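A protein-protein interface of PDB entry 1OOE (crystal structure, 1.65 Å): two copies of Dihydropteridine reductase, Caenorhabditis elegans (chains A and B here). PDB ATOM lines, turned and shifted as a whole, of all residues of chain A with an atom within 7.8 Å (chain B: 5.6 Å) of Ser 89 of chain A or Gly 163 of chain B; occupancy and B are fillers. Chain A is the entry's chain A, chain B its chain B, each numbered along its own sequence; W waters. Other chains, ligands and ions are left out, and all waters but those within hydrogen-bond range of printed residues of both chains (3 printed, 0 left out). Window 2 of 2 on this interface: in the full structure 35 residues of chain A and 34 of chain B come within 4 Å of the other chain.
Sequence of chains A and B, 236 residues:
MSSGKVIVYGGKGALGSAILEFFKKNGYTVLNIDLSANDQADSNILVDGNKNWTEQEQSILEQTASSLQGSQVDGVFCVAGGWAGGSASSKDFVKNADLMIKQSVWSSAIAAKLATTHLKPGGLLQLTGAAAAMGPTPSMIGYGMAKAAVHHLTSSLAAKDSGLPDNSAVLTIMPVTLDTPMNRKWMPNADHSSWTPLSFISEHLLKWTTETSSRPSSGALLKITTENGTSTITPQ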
ATOM      1  N   GLY A  86       8.311 -19.244   9.700  1.00  0.00           N
ATOM      2  CA  GLY A  86       8.389 -18.931  11.116  1.00  0.00           C
ATOM      3  C   GLY A  86       7.160 -18.286  11.730  1.00  0.00           C
ATOM      4  O   GLY A  86       6.602 -17.333  11.179  1.00  0.00           O
ATOM      5  N   SER A  87       6.727 -18.812  12.874  1.00  0.00           N
ATOM      6  CA  SER A  87       5.580 -18.252  13.577  1.00  0.00           C
ATOM      7  C   SER A  87       6.115 -17.084  14.399  1.00  0.00           C
ATOM      8  O   SER A  87       7.312 -16.804  14.368  1.00  0.00           O
ATOM      9  CB  SER A  87       4.953 -19.291  14.511  1.00  0.00           C
ATOM     10  OG  SER A  87       5.805 -19.562  15.614  1.00  0.00           O
ATOM     11  N   ALA A  88       5.241 -16.407  15.137  1.00  0.00           N
ATOM     12  CA  ALA A  88       5.670 -15.274  15.952  1.00  0.00           C
ATOM     13  C   ALA A  88       6.626 -15.681  17.074  1.00  0.00           C
ATOM     14  O   ALA A  88       7.401 -14.859  17.566  1.00  0.00           O
ATOM     15  CB  ALA A  88       4.455 -14.554  16.534  1.00  0.00           C
ATOM     16  N   SER A  89       6.580 -16.945  17.480  1.00  0.00           N
ATOM     17  CA  SER A  89       7.462 -17.405  18.547  1.00  0.00           C
ATOM     18  C   SER A  89       8.828 -17.849  18.018  1.00  0.00           C
ATOM     19  O   SER A  89       9.731 -18.166  18.794  1.00  0.00           O
ATOM     20  CB  SER A  89       6.794 -18.537  19.335  1.00  0.00           C
ATOM     21  OG  SER A  89       6.417 -19.605  18.488  1.00  0.00           O
ATOM     22  N   SER A  90       8.981 -17.870  16.698  1.00  0.00           N
ATOM     23  CA  SER A  90      10.248 -18.252  16.087  1.00  0.00           C
ATOM     24  C   SER A  90      11.305 -17.202  16.393  1.00  0.00           C
ATOM     25  O   SER A  90      11.006 -16.008  16.447  1.00  0.00           O
ATOM     26  CB  SER A  90      10.102 -18.373  14.570  1.00  0.00           C
ATOM     27  OG  SER A  90      11.379 -18.406  13.956  1.00  0.00           O
ATOM     28  N   LYS A  91      12.541 -17.645  16.588  1.00  0.00           N
ATOM     29  CA  LYS A  91      13.629 -16.724  16.885  1.00  0.00           C
ATOM     30  C   LYS A  91      13.820 -15.735  15.737  1.00  0.00           C
ATOM     31  O   LYS A  91      14.135 -14.566  15.962  1.00  0.00           O
ATOM     32  CB  LYS A  91      14.929 -17.498  17.124  1.00  0.00           C
ATOM     33  CG  LYS A  91      16.119 -16.613  17.467  1.00  0.00           C
ATOM     34  CD  LYS A  91      17.351 -17.431  17.828  1.00  0.00           C
ATOM     35  CE  LYS A  91      17.831 -18.283  16.662  1.00  0.00           C
ATOM     36  NZ  LYS A  91      19.044 -19.067  17.031  1.00  0.00           N
ATOM     37  N   ASP A  92      13.614 -16.208  14.511  1.00  0.00           N
ATOM     38  CA  ASP A  92      13.780 -15.365  13.333  1.00  0.00           C
ATOM     39  C   ASP A  92      12.468 -14.870  12.722  1.00  0.00           C
ATOM     40  O   ASP A  92      12.391 -14.655  11.514  1.00  0.00           O
ATOM     41  CB  ASP A  92      14.581 -16.109  12.260  1.00  0.00           C
ATOM     42  CG  ASP A  92      15.949 -16.541  12.746  1.00  0.00           C
ATOM     43  OD1 ASP A  92      16.663 -15.709  13.341  1.00  0.00           O
ATOM     44  OD2 ASP A  92      16.313 -17.714  12.523  1.00  0.00           O
ATOM     45  N   PHE A  93      11.443 -14.688  13.551  1.00  0.00           N
ATOM     46  CA  PHE A  93      10.152 -14.203  13.064  1.00  0.00           C
ATOM     47  C   PHE A  93      10.331 -12.885  12.310  1.00  0.00           C
ATOM     48  O   PHE A  93       9.902 -12.757  11.159  1.00  0.00           O
ATOM     49  CB  PHE A  93       9.175 -14.019  14.243  1.00  0.00           C
ATOM     50  CG  PHE A  93       7.984 -13.134  13.933  1.00  0.00           C
ATOM     51  CD1 PHE A  93       7.170 -13.383  12.830  1.00  0.00           C
ATOM     52  CD2 PHE A  93       7.676 -12.057  14.759  1.00  0.00           C
ATOM     53  CE1 PHE A  93       6.069 -12.571  12.554  1.00  0.00           C
ATOM     54  CE2 PHE A  93       6.576 -11.235  14.494  1.00  0.00           C
ATOM     55  CZ  PHE A  93       5.771 -11.495  13.388  1.00  0.00           C
ATOM     56  N   PRO A 138      -0.180 -18.903  10.199  1.00  0.00           N
ATOM     57  CA  PRO A 138       0.531 -18.882  11.482  1.00  0.00           C
ATOM     58  C   PRO A 138       1.939 -19.490  11.509  1.00  0.00           C
ATOM     59  O   PRO A 138       2.759 -19.105  12.345  1.00  0.00           O
ATOM     60  CB  PRO A 138      -0.431 -19.609  12.422  1.00  0.00           C
ATOM     61  CG  PRO A 138      -1.144 -20.562  11.507  1.00  0.00           C
ATOM     62  CD  PRO A 138      -1.420 -19.692  10.300  1.00  0.00           C
ATOM     63  N   ILE A 141       4.258 -16.470   9.130  1.00  0.00           N
ATOM     64  CA  ILE A 141       3.654 -15.148   9.222  1.00  0.00           C
ATOM     65  C   ILE A 141       4.253 -14.066   8.327  1.00  0.00           C
ATOM     66  O   ILE A 141       3.510 -13.313   7.697  1.00  0.00           O
ATOM     67  CB  ILE A 141       3.639 -14.684  10.699  1.00  0.00           C
ATOM     68  CG1 ILE A 141       2.785 -15.663  11.513  1.00  0.00           C
ATOM     69  CG2 ILE A 141       3.082 -13.272  10.813  1.00  0.00           C
ATOM     70  CD1 ILE A 141       2.665 -15.337  12.998  1.00  0.00           C
ATOM     71  N   LYS B 113       5.592  -9.554  18.765  1.00  0.00           N
ATOM     72  CA  LYS B 113       6.711 -10.269  19.375  1.00  0.00           C
ATOM     73  C   LYS B 113       6.700 -10.007  20.875  1.00  0.00           C
ATOM     74  O   LYS B 113       6.982 -10.899  21.674  1.00  0.00           O
ATOM     75  CB  LYS B 113       8.042  -9.796  18.781  1.00  0.00           C
ATOM     76  CG  LYS B 113       9.241 -10.658  19.168  1.00  0.00           C
ATOM     77  CD  LYS B 113       9.193 -12.022  18.489  1.00  0.00           C
ATOM     78  CE  LYS B 113      10.291 -12.937  19.011  1.00  0.00           C
ATOM     79  NZ  LYS B 113      10.360 -14.203  18.233  1.00  0.00           N
ATOM     80  N   THR B 116       3.987 -12.333  22.394  1.00  0.00           N
ATOM     81  CA  THR B 116       4.342 -13.747  22.515  1.00  0.00           C
ATOM     82  C   THR B 116       5.276 -13.961  23.704  1.00  0.00           C
ATOM     83  O   THR B 116       5.224 -14.992  24.378  1.00  0.00           O
ATOM     84  CB  THR B 116       5.042 -14.294  21.238  1.00  0.00           C
ATOM     85  OG1 THR B 116       6.347 -13.714  21.116  1.00  0.00           O
ATOM     86  CG2 THR B 116       4.228 -13.966  19.999  1.00  0.00           C
ATOM     87  N   ALA B 159      -4.852 -17.323  14.758  1.00  0.00           N
ATOM     88  CA  ALA B 159      -4.886 -18.763  14.530  1.00  0.00           C
ATOM     89  C   ALA B 159      -4.087 -19.527  15.583  1.00  0.00           C
ATOM     90  O   ALA B 159      -3.192 -18.979  16.222  1.00  0.00           O
ATOM     91  CB  ALA B 159      -4.348 -19.079  13.136  1.00  0.00           C
ATOM     92  N   ASP B 161      -1.392 -21.905  17.334  1.00  0.00           N
ATOM     93  CA  ASP B 161       0.042 -22.077  17.138  1.00  0.00           C
ATOM     94  C   ASP B 161       0.774 -20.911  16.476  1.00  0.00           C
ATOM     95  O   ASP B 161       1.837 -21.094  15.888  1.00  0.00           O
ATOM     96  CB  ASP B 161       0.307 -23.368  16.360  1.00  0.00           C
ATOM     97  CG  ASP B 161      -0.182 -24.594  17.100  1.00  0.00           C
ATOM     98  OD1 ASP B 161       0.184 -24.751  18.284  1.00  0.00           O
ATOM     99  OD2 ASP B 161      -0.928 -25.400  16.507  1.00  0.00           O
ATOM    100  N   SER B 162       0.208 -19.713  16.584  1.00  0.00           N
ATOM    101  CA  SER B 162       0.832 -18.522  16.014  1.00  0.00           C
ATOM    102  C   SER B 162       1.966 -18.062  16.926  1.00  0.00           C
ATOM    103  O   SER B 162       2.862 -17.338  16.506  1.00  0.00           O
ATOM    104  CB  SER B 162      -0.184 -17.391  15.912  1.00  0.00           C
ATOM    105  OG  SER B 162      -0.543 -16.944  17.211  1.00  0.00           O
ATOM    106  N   GLY B 163       1.913 -18.477  18.186  1.00  0.00           N
ATOM    107  CA  GLY B 163       2.940 -18.065  19.118  1.00  0.00           C
ATOM    108  C   GLY B 163       2.376 -17.231  20.251  1.00  0.00           C
ATOM    109  O   GLY B 163       3.018 -17.096  21.291  1.00  0.00           O
ATOM    110  N   LEU B 164       1.190 -16.655  20.053  1.00  0.00           N
ATOM    111  CA  LEU B 164       0.568 -15.857  21.106  1.00  0.00           C
ATOM    112  C   LEU B 164       0.184 -16.769  22.271  1.00  0.00           C
ATOM    113  O   LEU B 164      -0.061 -17.959  22.086  1.00  0.00           O
ATOM    114  CB  LEU B 164      -0.674 -15.128  20.584  1.00  0.00           C
ATOM    115  CG  LEU B 164      -0.401 -13.934  19.665  1.00  0.00           C
ATOM    116  CD1 LEU B 164      -1.713 -13.270  19.293  1.00  0.00           C
ATOM    117  CD2 LEU B 164       0.520 -12.937  20.365  1.00  0.00           C
ATOM    118  N   PRO B 165       0.125 -16.218  23.489  1.00  0.00           N
ATOM    119  CA  PRO B 165      -0.230 -17.029  24.658  1.00  0.00           C
ATOM    120  C   PRO B 165      -1.606 -17.686  24.607  1.00  0.00           C
ATOM    121  O   PRO B 165      -2.510 -17.220  23.911  1.00  0.00           O
ATOM    122  CB  PRO B 165      -0.084 -16.047  25.821  1.00  0.00           C
ATOM    123  CG  PRO B 165      -0.308 -14.709  25.184  1.00  0.00           C
ATOM    124  CD  PRO B 165       0.410 -14.826  23.873  1.00  0.00           C
HETATM  125  O   HOH W   1       4.284 -21.420  17.077  1.00  0.00           O
HETATM  126  O   HOH W   2      11.766 -16.161  19.769  1.00  0.00           O
HETATM  127  O   HOH W   3      11.685 -12.641  16.047  1.00  0.00           O
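Water W1 lies within hydrogen-bond range of O of Asp 161 of chain B (2.7 Å), OG of Ser 87 of chain A (2.8 Å) and OG of Ser 89 of chain A (3.1 Å). Water W2 lies within hydrogen-bond range of the side-chain amino group of Lys 113 of chain B (2.9 Å), the backbone carbonyl oxygen of Ser 89 of chain A (3.0 Å) and the backbone carbonyl oxygen of Ser 90 of chain A (3.4 Å). Water W3 lies within hydrogen-bond range of the side-chain amino group (NZ) of Lys 113 of chain B (3.0 Å), the backbone carbonyl oxygen (O) of Lys 91 of chain A (3.1 Å), the backbone NH (N) of Phe 93 of chain A (3.2 Å) and the backbone carbonyl oxygen (O) of Ser 90 of chain A (3.5 Å).
The side-chain hydroxyl of Ser 87 of chain A lies within hydrogen-bond range of the side-chain hydroxyl of Ser 89 of chain A, at 2.9 Å. The backbone carbonyl oxygen (O) of Lys 113 of chain B is in hydrogen-bond range of the side-chain hydroxyl (OG1) of Thr 116 of chain B (2.9 Å). OG of Ser 90 of chain A sits close to N of Asp 92 of chain A, at 3.2 Å. OG of Ser 162 of chain B lies within hydrogen-bond range of N of Leu 164 of chain B. The backbone carbonyl oxygen (O) of Ala 159 of chain B sits close to the side-chain hydroxyl (OG) of Ser 162 of chain B (3.5 Å).
Printed residues of chain B within 4 Å of Ser 87 of chain A: Asp 161 (3.9 Å) and Ser 162 (3.5 Å). Printed residues of chain B within 4 Å of Ser 89 of chain A: Lys 113 (3.96 Å), Ser 162 (3.9 Å) and Gly 163 (3.9 Å). Lys 91 of chain A touches none of the printed residues of chain B. Of the printed residues of chain A, Lys 113 of chain B touches Ala 88, Ser 89 and Ser 90. Of chain A, only Ser 87, Ala 88, Ser 89 and Pro 138 come within 4 Å of Ser 162 of chain B. Of chain A, only Ser 89 (3.9 Å) comes within 4 Å of Gly 163 of chain B. The nearest printed residue of chain B that does not touch Ser 89 of chain A is Thr 116 of chain B (4.6 Å). The nearest residue of chain A that does not touch Gly 163 of chain B is Ala 88 of chain A (4.6 Å). The nearest printed residue of chain B that does not touch Pro 138 of chain A is Asp 161 of chain B (4.2 Å).
Among the printed residues, pairs that only touch across the chains: Ser 87 of chain A with Ser 162 of chain B, Ala 88 of chain A with Thr 116 of chain B, Ser 87 of chain A with Asp 161 of chain B, Ser 89 of chain A with Gly 163 of chain B, Ser 89 of chain A with Ser 162 of chain B, Pro 138 of chain A with Ala 159 of chain B, Pro 138 of chain A with Ser 162 of chain B and Ser 89 of chain A with Lys 113 of chain B.
N of Ala 88 of chain A is in hydrogen-bond range of O of Ser 162 of chain B (2.9 Å). The backbone carbonyl oxygen (O) of Ser 90 of chain A is in hydrogen-bond range of the side-chain amino group (NZ) of Lys 113 of chain B (2.6 Å). The side-chain amino group of Lys 113 of chain B is in hydrogen-bond range of the backbone carbonyl oxygen of Ala 88 of chain A, 3.1 Å away.
No position is printed for both chains. Of the 11 pairs that touch across the chains among the printed residues, none has its exchanged pair printed and touching as well.
Printed residues of chain B that touch a printed residue of chain A: Lys 113, Thr 116, Ala 159, Asp 161, Ser 162 and Gly 163. Printed residues of chain A that touch a printed residue of chain B: Ser 87, Ala 88, Ser 89, Ser 90 and Pro 138. Hydrophobic or aromatic side chains of chain A that line the printed part of chain B: Ala 88 and Pro 138. Among the printed residues, 11 pairs touch across the chains. Among the printed residues, no Asp or Glu carboxylate lies within 4 Å of a Lys or Arg side-chain nitrogen of the other chain.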
